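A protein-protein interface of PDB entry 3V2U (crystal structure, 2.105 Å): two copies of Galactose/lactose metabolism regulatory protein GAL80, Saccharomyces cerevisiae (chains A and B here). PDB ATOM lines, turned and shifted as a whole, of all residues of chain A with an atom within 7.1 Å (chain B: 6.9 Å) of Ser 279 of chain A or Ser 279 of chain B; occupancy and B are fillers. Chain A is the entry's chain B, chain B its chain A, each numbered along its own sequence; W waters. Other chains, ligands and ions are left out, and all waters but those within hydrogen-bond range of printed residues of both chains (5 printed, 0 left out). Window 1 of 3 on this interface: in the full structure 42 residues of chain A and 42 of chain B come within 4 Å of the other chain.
Water W1 lies within hydrogen-bond range of the side-chain hydroxyl of Ser 279 of chain B (2.6 Å) and the side-chain hydroxyl of Ser 279 of chain A (2.7 Å). Water W4 lies within hydrogen-bond range of the side-chain hydroxyl (OG) of Ser 281 of chain A (2.6 Å), the backbone carbonyl oxygen (O) of Ile 179 of chain B (2.8 Å) and the side-chain carboxylate (OE2) of Glu 180 of chain B (2.9 Å). Water W3 lies within hydrogen-bond range of OG of Ser 281 of chain B (2.6 Å), OE2 of Glu 180 of chain A (2.8 Å) and O of Ile 179 of chain A (2.8 Å). Water W5 lies within hydrogen-bond range of the side-chain amide nitrogen (NE2) of Gln 268 of chain B, the side-chain hydroxyl (OG) of Ser 279 of chain B, the backbone carbonyl oxygen (O) of Cys 280 of chain A and the backbone carbonyl oxygen (O) of Phe 267 of chain A. Water W2 lies within hydrogen-bond range of the side-chain hydroxyl (OG) of Ser 279 of chain A (2.7 Å), the side-chain amide nitrogen (NE2) of Gln 268 of chain A (2.8 Å), the backbone carbonyl oxygen (O) of Cys 280 of chain B (3.0 Å) and the backbone carbonyl oxygen (O) of Phe 267 of chain B (3.3 Å).
O of Ser 279 of chain B is in hydrogen-bond range of N of Ile 181 of chain B, at 2.8 Å. The backbone carbonyl oxygen of Ile 181 of chain B lies within hydrogen-bond range of the backbone NH of Ser 281 of chain B (3.1 Å). The backbone carbonyl oxygen (O) of Gly 269 of chain B is in hydrogen-bond range of the backbone NH (N) of Val 278 of chain B (2.9 Å). The backbone carbonyl oxygen (O) of Ile 181 of chain A lies within hydrogen-bond range of the backbone NH (N) of Ser 281 of chain A (3.1 Å). The backbone NH (N) of Cys 280 of chain A is in hydrogen-bond range of the backbone carbonyl oxygen (O) of Phe 267 of chain A (2.6 Å). The backbone carbonyl oxygen (O) of Gly 269 of chain A lies within hydrogen-bond range of the backbone NH (N) of Val 278 of chain A, 2.8 Å away.
Pro 277 of chain B touches His 264 of chain A. Leu 266 of chain A touches Gln 268 of chain B. Leu 266 of chain A touches Pro 277 of chain B. CD1 of Leu 266 of chain A touches O of Val 278 of chain B, 3.6 Å away. NE2 of Gln 268 of chain A touches CB of Leu 266 of chain B (3.4 Å). CD of Gln 268 of chain B touches CD of Gln 268 of chain A, at 3.5 Å. His 264 of chain B touches Pro 277 of chain A. Cys 280 of chain B touches Ser 279 of chain A (O to OG, 3.9 Å). Ser 279 of chain A touches Ser 281 of chain B (CB to CB, 3.8 Å). Ser 279 of chain B touches Ser 281 of chain A (CB to CB, 3.9 Å).
The backbone NH of Phe 267 of chain B lies close to the side-chain amide nitrogen of Gln 268 of chain A (3.4 Å). The side-chain amide nitrogen (NE2) of Gln 268 of chain B lies close to the backbone NH (N) of Phe 267 of chain A (3.3 Å). The side-chain hydroxyl (OG) of Ser 279 of chain A sits at hydrogen-bond distance from the side-chain hydroxyl (OG) of Ser 279 of chain B, 3.4 Å away.
Of the 17 printed residues of chain B, 12 touch a printed residue of chain A. Along chain B the printed residues that touch a printed residue of chain A span positions 178 to 281. Printed residues of chain A that touch a printed residue of chain B: Ser 178, Glu 180, His 264, Leu 266, Phe 267, Gln 268, Gly 269, Pro 277, Val 278, Ser 279, Cys 280 and Ser 281. Hydrophobic or aromatic side chains of chain A within 4 Å of the printed part of chain B: His 264, Leu 266 and Pro 277. Among the printed residues, 24 pairs touch across the chains. Among the printed residues, no Asp or Glu carboxylate lies within 4 Å of a Lys or Arg side-chain nitrogen of the other chain.
Ser 178 of chain A touches His 264 of chain B, and with the chains exchanged His 264 of chain A touches Ser 178 of chain B. Glu 180 of chain A touches Ser 281 of chain B, and with the chains exchanged Ser 281 of chain A touches Glu 180 of chain B. Leu 266 of chain A touches Val 278 of chain B, and with the chains exchanged Val 278 of chain A touches Leu 266 of chain B. Ser 279 of chain A touches Cys 280 of chain B, and with the chains exchanged Cys 280 of chain A touches Ser 279 of chain B. 17 positions are printed for both chains.
Of the printed residues of chain B, Ser 178 of chain A touches His 264. Printed residues of chain B within 4 Å of Pro 277 of chain A: His 264 (3.6 Å) and Leu 266 (3.99 Å). Of the printed residues of chain B, Ser 279 of chain A touches Leu 266 (3.7 Å), Ser 279 (3.4 Å), Cys 280 (3.9 Å) and Ser 281 (3.8 Å). Of the printed residues of chain A, Phe 267 of chain B touches Gln 268 (3.4 Å). Of the printed residues of chain A, Gly 269 of chain B touches Leu 266 (3.7 Å). Of the printed residues of chain A, Ser 279 of chain B touches Leu 266 (3.7 Å), Ser 279 (3.4 Å), Cys 280 (3.9 Å) and Ser 281 (3.9 Å). The nearest printed residue of chain B that does not touch Ser 279 of chain A is Phe 267 of chain B (5.4 Å).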
ATOM      1  N   SER A 178      -8.156 -12.356   7.394  1.00  0.00           N
ATOM      2  CA  SER A 178      -8.713 -11.592   8.490  1.00  0.00           C
ATOM      3  C   SER A 178      -7.800 -11.682   9.698  1.00  0.00           C
ATOM      4  O   SER A 178      -6.934 -12.571   9.779  1.00  0.00           O
ATOM      5  CB  SER A 178     -10.124 -12.093   8.837  1.00  0.00           C
ATOM      6  OG  SER A 178     -10.122 -13.501   9.056  1.00  0.00           O
ATOM      7  N   ILE A 179      -8.001 -10.760  10.635  1.00  0.00           N
ATOM      8  CA  ILE A 179      -7.147 -10.650  11.817  1.00  0.00           C
ATOM      9  C   ILE A 179      -7.982 -10.291  13.037  1.00  0.00           C
ATOM     10  O   ILE A 179      -8.859  -9.436  12.947  1.00  0.00           O
ATOM     11  CB  ILE A 179      -6.076  -9.548  11.598  1.00  0.00           C
ATOM     12  CG1 ILE A 179      -5.166  -9.931  10.423  1.00  0.00           C
ATOM     13  CG2 ILE A 179      -5.285  -9.284  12.884  1.00  0.00           C
ATOM     14  CD1 ILE A 179      -4.256  -8.787   9.917  1.00  0.00           C
ATOM     15  N   GLU A 180      -7.722 -10.969  14.160  1.00  0.00           N
ATOM     16  CA  GLU A 180      -8.296 -10.629  15.460  1.00  0.00           C
ATOM     17  C   GLU A 180      -7.183 -10.376  16.457  1.00  0.00           C
ATOM     18  O   GLU A 180      -6.190 -11.111  16.512  1.00  0.00           O
ATOM     19  CB  GLU A 180      -9.170 -11.767  16.025  1.00  0.00           C
ATOM     20  CG  GLU A 180     -10.363 -12.110  15.175  1.00  0.00           C
ATOM     21  CD  GLU A 180     -10.039 -13.166  14.157  1.00  0.00           C
ATOM     22  OE1 GLU A 180      -9.665 -14.282  14.591  1.00  0.00           O
ATOM     23  OE2 GLU A 180     -10.145 -12.878  12.937  1.00  0.00           O
ATOM     24  N   ILE A 181      -7.356  -9.325  17.243  1.00  0.00           N
ATOM     25  CA  ILE A 181      -6.399  -8.975  18.276  1.00  0.00           C
ATOM     26  C   ILE A 181      -7.141  -8.822  19.590  1.00  0.00           C
ATOM     27  O   ILE A 181      -8.246  -8.277  19.642  1.00  0.00           O
ATOM     28  CB  ILE A 181      -5.651  -7.690  17.935  1.00  0.00           C
ATOM     29  CG1 ILE A 181      -4.756  -7.937  16.716  1.00  0.00           C
ATOM     30  CG2 ILE A 181      -4.796  -7.228  19.125  1.00  0.00           C
ATOM     31  CD1 ILE A 181      -3.987  -6.714  16.261  1.00  0.00           C
ATOM     32  N   ALA A 182      -6.545  -9.347  20.647  1.00  0.00           N
ATOM     33  CA  ALA A 182      -7.070  -9.135  21.988  1.00  0.00           C
ATOM     34  C   ALA A 182      -5.887  -8.767  22.873  1.00  0.00           C
ATOM     35  O   ALA A 182      -4.840  -9.411  22.813  1.00  0.00           O
ATOM     36  CB  ALA A 182      -7.762 -10.364  22.483  1.00  0.00           C
ATOM     37  N   PHE A 229      -3.586   1.424   7.901  1.00  0.00           N
ATOM     38  CA  PHE A 229      -5.033   1.255   7.830  1.00  0.00           C
ATOM     39  C   PHE A 229      -5.665   2.095   6.739  1.00  0.00           C
ATOM     40  O   PHE A 229      -5.152   3.157   6.373  1.00  0.00           O
ATOM     41  CB  PHE A 229      -5.685   1.533   9.191  1.00  0.00           C
ATOM     42  CG  PHE A 229      -5.539   0.391  10.157  1.00  0.00           C
ATOM     43  CD1 PHE A 229      -4.376   0.241  10.907  1.00  0.00           C
ATOM     44  CD2 PHE A 229      -6.536  -0.564  10.273  1.00  0.00           C
ATOM     45  CE1 PHE A 229      -4.223  -0.827  11.770  1.00  0.00           C
ATOM     46  CE2 PHE A 229      -6.393  -1.642  11.146  1.00  0.00           C
ATOM     47  CZ  PHE A 229      -5.234  -1.769  11.896  1.00  0.00           C
ATOM     48  N   HIS A 264     -11.614   0.440  28.504  1.00  0.00           N
ATOM     49  CA  HIS A 264     -11.803  -0.486  27.383  1.00  0.00           C
ATOM     50  C   HIS A 264     -11.685   0.196  26.034  1.00  0.00           C
ATOM     51  O   HIS A 264     -11.999   1.384  25.886  1.00  0.00           O
ATOM     52  CB  HIS A 264     -13.156  -1.234  27.455  1.00  0.00           C
ATOM     53  CG  HIS A 264     -13.098  -2.621  26.888  1.00  0.00           C
ATOM     54  ND1 HIS A 264     -13.338  -2.897  25.545  1.00  0.00           N
ATOM     55  CD2 HIS A 264     -12.801  -3.808  27.458  1.00  0.00           C
ATOM     56  CE1 HIS A 264     -13.204  -4.186  25.331  1.00  0.00           C
ATOM     57  NE2 HIS A 264     -12.861  -4.771  26.471  1.00  0.00           N
ATOM     58  N   LEU A 265     -11.236  -0.570  25.051  1.00  0.00           N
ATOM     59  CA  LEU A 265     -11.176  -0.104  23.683  1.00  0.00           C
ATOM     60  C   LEU A 265     -11.719  -1.154  22.736  1.00  0.00           C
ATOM     61  O   LEU A 265     -11.243  -2.301  22.720  1.00  0.00           O
ATOM     62  CB  LEU A 265      -9.730   0.211  23.282  1.00  0.00           C
ATOM     63  CG  LEU A 265      -9.519   0.496  21.786  1.00  0.00           C
ATOM     64  CD1 LEU A 265     -10.243   1.771  21.326  1.00  0.00           C
ATOM     65  CD2 LEU A 265      -8.003   0.571  21.470  1.00  0.00           C
ATOM     66  N   LEU A 266     -12.720  -0.773  21.951  1.00  0.00           N
ATOM     67  CA  LEU A 266     -13.086  -1.585  20.797  1.00  0.00           C
ATOM     68  C   LEU A 266     -12.562  -0.901  19.540  1.00  0.00           C
ATOM     69  O   LEU A 266     -12.776   0.298  19.342  1.00  0.00           O
ATOM     70  CB  LEU A 266     -14.615  -1.764  20.680  1.00  0.00           C
ATOM     71  CG  LEU A 266     -15.321  -2.407  21.876  1.00  0.00           C
ATOM     72  CD1 LEU A 266     -16.861  -2.292  21.746  1.00  0.00           C
ATOM     73  CD2 LEU A 266     -14.897  -3.871  22.011  1.00  0.00           C
ATOM     74  N   PHE A 267     -11.916  -1.672  18.677  1.00  0.00           N
ATOM     75  CA  PHE A 267     -11.336  -1.129  17.449  1.00  0.00           C
ATOM     76  C   PHE A 267     -11.544  -2.112  16.321  1.00  0.00           C
ATOM     77  O   PHE A 267     -11.275  -3.316  16.455  1.00  0.00           O
ATOM     78  CB  PHE A 267      -9.841  -0.874  17.642  1.00  0.00           C
ATOM     79  CG  PHE A 267      -9.102  -0.492  16.377  1.00  0.00           C
ATOM     80  CD1 PHE A 267      -8.900   0.845  16.054  1.00  0.00           C
ATOM     81  CD2 PHE A 267      -8.594  -1.471  15.526  1.00  0.00           C
ATOM     82  CE1 PHE A 267      -8.201   1.215  14.902  1.00  0.00           C
ATOM     83  CE2 PHE A 267      -7.891  -1.116  14.368  1.00  0.00           C
ATOM     84  CZ  PHE A 267      -7.692   0.237  14.061  1.00  0.00           C
ATOM     85  N   GLN A 268     -12.013  -1.607  15.197  1.00  0.00           N
ATOM     86  CA  GLN A 268     -12.115  -2.449  14.021  1.00  0.00           C
ATOM     87  C   GLN A 268     -11.765  -1.598  12.816  1.00  0.00           C
ATOM     88  O   GLN A 268     -11.935  -0.373  12.836  1.00  0.00           O
ATOM     89  CB  GLN A 268     -13.515  -3.091  13.903  1.00  0.00           C
ATOM     90  CG  GLN A 268     -14.642  -2.130  13.509  1.00  0.00           C
ATOM     91  CD  GLN A 268     -16.059  -2.696  13.750  1.00  0.00           C
ATOM     92  OE1 GLN A 268     -17.063  -2.034  13.456  1.00  0.00           O
ATOM     93  NE2 GLN A 268     -16.139  -3.900  14.289  1.00  0.00           N
ATOM     94  N   GLY A 269     -11.256  -2.243  11.774  1.00  0.00           N
ATOM     95  CA  GLY A 269     -10.898  -1.528  10.564  1.00  0.00           C
ATOM     96  C   GLY A 269     -10.301  -2.433   9.499  1.00  0.00           C
ATOM     97  O   GLY A 269     -10.358  -3.673   9.590  1.00  0.00           O
ATOM     98  N   VAL A 276      -7.971  -5.839   4.404  1.00  0.00           N
ATOM     99  CA  VAL A 276      -8.071  -6.908   5.392  1.00  0.00           C
ATOM    100  C   VAL A 276      -8.833  -6.488   6.639  1.00  0.00           C
ATOM    101  O   VAL A 276      -8.474  -5.510   7.286  1.00  0.00           O
ATOM    102  CB  VAL A 276      -6.680  -7.386   5.859  1.00  0.00           C
ATOM    103  CG1 VAL A 276      -6.835  -8.564   6.850  1.00  0.00           C
ATOM    104  CG2 VAL A 276      -5.809  -7.771   4.664  1.00  0.00           C
ATOM    105  N   PRO A 277      -9.887  -7.244   6.986  1.00  0.00           N
ATOM    106  CA  PRO A 277     -10.667  -7.000   8.206  1.00  0.00           C
ATOM    107  C   PRO A 277      -9.837  -7.232   9.458  1.00  0.00           C
ATOM    108  O   PRO A 277      -9.229  -8.294   9.589  1.00  0.00           O
ATOM    109  CB  PRO A 277     -11.764  -8.074   8.157  1.00  0.00           C
ATOM    110  CG  PRO A 277     -11.746  -8.618   6.803  1.00  0.00           C
ATOM    111  CD  PRO A 277     -10.396  -8.391   6.215  1.00  0.00           C
ATOM    112  N   VAL A 278      -9.860  -6.275  10.379  1.00  0.00           N
ATOM    113  CA  VAL A 278      -9.149  -6.393  11.639  1.00  0.00           C
ATOM    114  C   VAL A 278     -10.115  -6.073  12.773  1.00  0.00           C
ATOM    115  O   VAL A 278     -10.750  -5.013  12.770  1.00  0.00           O
ATOM    116  CB  VAL A 278      -7.962  -5.380  11.705  1.00  0.00           C
ATOM    117  CG1 VAL A 278      -7.233  -5.496  13.024  1.00  0.00           C
ATOM    118  CG2 VAL A 278      -7.004  -5.584  10.504  1.00  0.00           C
ATOM    119  N   SER A 279     -10.214  -6.980  13.741  1.00  0.00           N
ATOM    120  CA  SER A 279     -11.113  -6.798  14.885  1.00  0.00           C
ATOM    121  C   SER A 279     -10.257  -6.782  16.134  1.00  0.00           C
ATOM    122  O   SER A 279      -9.440  -7.670  16.325  1.00  0.00           O
ATOM    123  CB  SER A 279     -12.090  -7.979  14.968  1.00  0.00           C
ATOM    124  OG  SER A 279     -12.957  -7.855  16.073  1.00  0.00           O
ATOM    125  N   CYS A 280     -10.430  -5.765  16.975  1.00  0.00           N
ATOM    126  CA  CYS A 280      -9.645  -5.657  18.201  1.00  0.00           C
ATOM    127  C   CYS A 280     -10.490  -5.359  19.433  1.00  0.00           C
ATOM    128  O   CYS A 280     -11.467  -4.597  19.389  1.00  0.00           O
ATOM    129  CB  CYS A 280      -8.574  -4.569  18.068  1.00  0.00           C
ATOM    130  SG  CYS A 280      -7.451  -4.766  16.679  1.00  0.00           S
ATOM    131  N   SER A 281     -10.096  -5.959  20.544  1.00  0.00           N
ATOM    132  CA  SER A 281     -10.695  -5.641  21.826  1.00  0.00           C
ATOM    133  C   SER A 281      -9.572  -5.561  22.844  1.00  0.00           C
ATOM    134  O   SER A 281      -8.831  -6.530  23.035  1.00  0.00           O
ATOM    135  CB  SER A 281     -11.707  -6.713  22.242  1.00  0.00           C
ATOM    136  OG  SER A 281     -12.321  -6.344  23.469  1.00  0.00           O
ATOM    137  N   PHE A 282      -9.450  -4.409  23.495  1.00  0.00           N
ATOM    138  CA  PHE A 282      -8.481  -4.217  24.570  1.00  0.00           C
ATOM    139  C   PHE A 282      -9.161  -4.000  25.909  1.00  0.00           C
ATOM    140  O   PHE A 282      -9.833  -2.981  26.129  1.00  0.00           O
ATOM    141  CB  PHE A 282      -7.546  -3.044  24.249  1.00  0.00           C
ATOM    142  CG  PHE A 282      -6.344  -3.451  23.449  1.00  0.00           C
ATOM    143  CD1 PHE A 282      -5.138  -3.697  24.074  1.00  0.00           C
ATOM    144  CD2 PHE A 282      -6.429  -3.612  22.078  1.00  0.00           C
ATOM    145  CE1 PHE A 282      -4.035  -4.077  23.342  1.00  0.00           C
ATOM    146  CE2 PHE A 282      -5.330  -3.996  21.347  1.00  0.00           C
ATOM    147  CZ  PHE A 282      -4.132  -4.230  21.983  1.00  0.00           C
ATOM    148  N   SER B 178     -16.990  -7.339  29.685  1.00  0.00           N
ATOM    149  CA  SER B 178     -16.752  -7.257  28.249  1.00  0.00           C
ATOM    150  C   SER B 178     -16.998  -8.595  27.600  1.00  0.00           C
ATOM    151  O   SER B 178     -16.988  -9.632  28.277  1.00  0.00           O
ATOM    152  CB  SER B 178     -15.316  -6.763  27.944  1.00  0.00           C
ATOM    153  OG  SER B 178     -14.342  -7.513  28.659  1.00  0.00           O
ATOM    154  N   ILE B 179     -17.219  -8.569  26.287  1.00  0.00           N
ATOM    155  CA  ILE B 179     -17.603  -9.761  25.548  1.00  0.00           C
ATOM    156  C   ILE B 179     -16.915  -9.807  24.195  1.00  0.00           C
ATOM    157  O   ILE B 179     -16.864  -8.801  23.500  1.00  0.00           O
ATOM    158  CB  ILE B 179     -19.145  -9.783  25.318  1.00  0.00           C
ATOM    159  CG1 ILE B 179     -19.867  -9.905  26.666  1.00  0.00           C
ATOM    160  CG2 ILE B 179     -19.511 -10.898  24.356  1.00  0.00           C
ATOM    161  CD1 ILE B 179     -21.401  -9.838  26.609  1.00  0.00           C
ATOM    162  N   GLU B 180     -16.391 -10.971  23.826  1.00  0.00           N
ATOM    163  CA  GLU B 180     -15.855 -11.214  22.488  1.00  0.00           C
ATOM    164  C   GLU B 180     -16.591 -12.380  21.871  1.00  0.00           C
ATOM    165  O   GLU B 180     -16.875 -13.368  22.552  1.00  0.00           O
ATOM    166  CB  GLU B 180     -14.359 -11.585  22.541  1.00  0.00           C
ATOM    167  CG  GLU B 180     -13.467 -10.469  23.049  1.00  0.00           C
ATOM    168  CD  GLU B 180     -13.217 -10.552  24.535  1.00  0.00           C
ATOM    169  OE1 GLU B 180     -12.751 -11.626  24.992  1.00  0.00           O
ATOM    170  OE2 GLU B 180     -13.482  -9.539  25.238  1.00  0.00           O
ATOM    171  N   ILE B 181     -16.874 -12.271  20.576  1.00  0.00           N
ATOM    172  CA  ILE B 181     -17.553 -13.310  19.842  1.00  0.00           C
ATOM    173  C   ILE B 181     -16.851 -13.509  18.521  1.00  0.00           C
ATOM    174  O   ILE B 181     -16.488 -12.551  17.842  1.00  0.00           O
ATOM    175  CB  ILE B 181     -19.033 -12.949  19.564  1.00  0.00           C
ATOM    176  CG1 ILE B 181     -19.822 -12.906  20.869  1.00  0.00           C
ATOM    177  CG2 ILE B 181     -19.662 -13.976  18.628  1.00  0.00           C
ATOM    178  CD1 ILE B 181     -21.230 -12.424  20.676  1.00  0.00           C
ATOM    179  N   ALA B 182     -16.644 -14.766  18.165  1.00  0.00           N
ATOM    180  CA  ALA B 182     -16.064 -15.093  16.865  1.00  0.00           C
ATOM    181  C   ALA B 182     -16.915 -16.202  16.277  1.00  0.00           C
ATOM    182  O   ALA B 182     -17.248 -17.153  16.969  1.00  0.00           O
ATOM    183  CB  ALA B 182     -14.615 -15.545  17.017  1.00  0.00           C
ATOM    184  N   HIS B 264     -17.300 -11.353   5.078  1.00  0.00           N
ATOM    185  CA  HIS B 264     -16.825 -11.042   6.437  1.00  0.00           C
ATOM    186  C   HIS B 264     -17.674  -9.990   7.107  1.00  0.00           C
ATOM    187  O   HIS B 264     -18.233  -9.122   6.446  1.00  0.00           O
ATOM    188  CB  HIS B 264     -15.338 -10.603   6.461  1.00  0.00           C
ATOM    189  CG  HIS B 264     -14.637 -10.944   7.740  1.00  0.00           C
ATOM    190  ND1 HIS B 264     -14.657 -10.120   8.850  1.00  0.00           N
ATOM    191  CD2 HIS B 264     -13.912 -12.035   8.093  1.00  0.00           C
ATOM    192  CE1 HIS B 264     -13.969 -10.688   9.828  1.00  0.00           C
ATOM    193  NE2 HIS B 264     -13.509 -11.851   9.395  1.00  0.00           N
ATOM    194  N   LEU B 265     -17.759 -10.069   8.425  1.00  0.00           N
ATOM    195  CA  LEU B 265     -18.470  -9.069   9.194  1.00  0.00           C
ATOM    196  C   LEU B 265     -17.673  -8.686  10.420  1.00  0.00           C
ATOM    197  O   LEU B 265     -17.331  -9.540  11.255  1.00  0.00           O
ATOM    198  CB  LEU B 265     -19.853  -9.575   9.637  1.00  0.00           C
ATOM    199  CG  LEU B 265     -20.590  -8.699  10.659  1.00  0.00           C
ATOM    200  CD1 LEU B 265     -21.042  -7.401  10.014  1.00  0.00           C
ATOM    201  CD2 LEU B 265     -21.803  -9.433  11.270  1.00  0.00           C
ATOM    202  N   LEU B 266     -17.387  -7.396  10.529  1.00  0.00           N
ATOM    203  CA  LEU B 266     -16.904  -6.832  11.779  1.00  0.00           C
ATOM    204  C   LEU B 266     -18.046  -6.103  12.449  1.00  0.00           C
ATOM    205  O   LEU B 266     -18.684  -5.226  11.845  1.00  0.00           O
ATOM    206  CB  LEU B 266     -15.759  -5.848  11.537  1.00  0.00           C
ATOM    207  CG  LEU B 266     -14.513  -6.425  10.839  1.00  0.00           C
ATOM    208  CD1 LEU B 266     -13.538  -5.317  10.425  1.00  0.00           C
ATOM    209  CD2 LEU B 266     -13.829  -7.417  11.753  1.00  0.00           C
ATOM    210  N   PHE B 267     -18.287  -6.439  13.706  1.00  0.00           N
ATOM    211  CA  PHE B 267     -19.364  -5.813  14.451  1.00  0.00           C
ATOM    212  C   PHE B 267     -18.831  -5.474  15.825  1.00  0.00           C
ATOM    213  O   PHE B 267     -18.148  -6.283  16.461  1.00  0.00           O
ATOM    214  CB  PHE B 267     -20.571  -6.762  14.536  1.00  0.00           C
ATOM    215  CG  PHE B 267     -21.668  -6.293  15.467  1.00  0.00           C
ATOM    216  CD1 PHE B 267     -22.745  -5.562  14.980  1.00  0.00           C
ATOM    217  CD2 PHE B 267     -21.635  -6.608  16.819  1.00  0.00           C
ATOM    218  CE1 PHE B 267     -23.768  -5.142  15.818  1.00  0.00           C
ATOM    219  CE2 PHE B 267     -22.654  -6.192  17.673  1.00  0.00           C
ATOM    220  CZ  PHE B 267     -23.728  -5.461  17.170  1.00  0.00           C
ATOM    221  N   GLN B 268     -19.110  -4.264  16.280  1.00  0.00           N
ATOM    222  CA  GLN B 268     -18.814  -3.932  17.656  1.00  0.00           C
ATOM    223  C   GLN B 268     -19.947  -3.064  18.179  1.00  0.00           C
ATOM    224  O   GLN B 268     -20.581  -2.332  17.419  1.00  0.00           O
ATOM    225  CB  GLN B 268     -17.418  -3.257  17.795  1.00  0.00           C
ATOM    226  CG  GLN B 268     -17.276  -1.924  17.073  1.00  0.00           C
ATOM    227  CD  GLN B 268     -15.825  -1.407  16.980  1.00  0.00           C
ATOM    228  OE1 GLN B 268     -15.597  -0.236  16.672  1.00  0.00           O
ATOM    229  NE2 GLN B 268     -14.852  -2.276  17.237  1.00  0.00           N
ATOM    230  N   GLY B 269     -20.214  -3.142  19.477  1.00  0.00           N
ATOM    231  CA  GLY B 269     -21.248  -2.314  20.048  1.00  0.00           C
ATOM    232  C   GLY B 269     -21.334  -2.436  21.546  1.00  0.00           C
ATOM    233  O   GLY B 269     -20.455  -3.023  22.180  1.00  0.00           O
ATOM    234  N   VAL B 276     -22.050  -2.469  28.088  1.00  0.00           N
ATOM    235  CA  VAL B 276     -21.013  -3.491  27.960  1.00  0.00           C
ATOM    236  C   VAL B 276     -20.415  -3.557  26.551  1.00  0.00           C
ATOM    237  O   VAL B 276     -21.144  -3.710  25.577  1.00  0.00           O
ATOM    238  CB  VAL B 276     -21.583  -4.882  28.318  1.00  0.00           C
ATOM    239  CG1 VAL B 276     -20.529  -5.956  28.096  1.00  0.00           C
ATOM    240  CG2 VAL B 276     -22.133  -4.887  29.774  1.00  0.00           C
ATOM    241  N   PRO B 277     -19.079  -3.445  26.439  1.00  0.00           N
ATOM    242  CA  PRO B 277     -18.392  -3.579  25.144  1.00  0.00           C
ATOM    243  C   PRO B 277     -18.481  -5.007  24.576  1.00  0.00           C
ATOM    244  O   PRO B 277     -18.188  -5.994  25.255  1.00  0.00           O
ATOM    245  CB  PRO B 277     -16.920  -3.267  25.472  1.00  0.00           C
ATOM    246  CG  PRO B 277     -16.905  -2.710  26.868  1.00  0.00           C
ATOM    247  CD  PRO B 277     -18.140  -3.216  27.556  1.00  0.00           C
ATOM    248  N   VAL B 278     -18.866  -5.101  23.314  1.00  0.00           N
ATOM    249  CA  VAL B 278     -18.983  -6.385  22.639  1.00  0.00           C
ATOM    250  C   VAL B 278     -18.202  -6.260  21.348  1.00  0.00           C
ATOM    251  O   VAL B 278     -18.419  -5.315  20.571  1.00  0.00           O
ATOM    252  CB  VAL B 278     -20.469  -6.690  22.284  1.00  0.00           C
ATOM    253  CG1 VAL B 278     -20.590  -7.986  21.452  1.00  0.00           C
ATOM    254  CG2 VAL B 278     -21.325  -6.760  23.551  1.00  0.00           C
ATOM    255  N   SER B 279     -17.290  -7.197  21.118  1.00  0.00           N
ATOM    256  CA  SER B 279     -16.482  -7.215  19.902  1.00  0.00           C
ATOM    257  C   SER B 279     -16.729  -8.511  19.154  1.00  0.00           C
ATOM    258  O   SER B 279     -16.598  -9.599  19.738  1.00  0.00           O
ATOM    259  CB  SER B 279     -15.002  -7.086  20.269  1.00  0.00           C
ATOM    260  OG  SER B 279     -14.171  -7.338  19.159  1.00  0.00           O
ATOM    261  N   CYS B 280     -17.087  -8.403  17.877  1.00  0.00           N
ATOM    262  CA  CYS B 280     -17.444  -9.575  17.076  1.00  0.00           C
ATOM    263  C   CYS B 280     -16.749  -9.601  15.714  1.00  0.00           C
ATOM    264  O   CYS B 280     -16.642  -8.582  15.022  1.00  0.00           O
ATOM    265  CB  CYS B 280     -18.958  -9.634  16.858  1.00  0.00           C
ATOM    266  SG  CYS B 280     -19.961  -9.503  18.351  1.00  0.00           S
ATOM    267  N   SER B 281     -16.285 -10.779  15.324  1.00  0.00           N
ATOM    268  CA  SER B 281     -15.778 -10.959  13.974  1.00  0.00           C
ATOM    269  C   SER B 281     -16.315 -12.259  13.406  1.00  0.00           C
ATOM    270  O   SER B 281     -16.141 -13.315  14.004  1.00  0.00           O
ATOM    271  CB  SER B 281     -14.242 -10.948  13.961  1.00  0.00           C
ATOM    272  OG  SER B 281     -13.738 -11.236  12.665  1.00  0.00           O
HETATM  273  O   HOH W   1     -12.770  -9.327  18.319  1.00  0.00           O
HETATM  274  O   HOH W   2     -15.019  -6.152  15.532  1.00  0.00           O
HETATM  275  O   HOH W   3     -11.300 -10.517  11.970  1.00  0.00           O
HETATM  276  O   HOH W   4     -14.719  -7.104  24.202  1.00  0.00           O
HETATM  277  O   HOH W   5     -13.940  -4.761  17.813  1.00  0.00           O
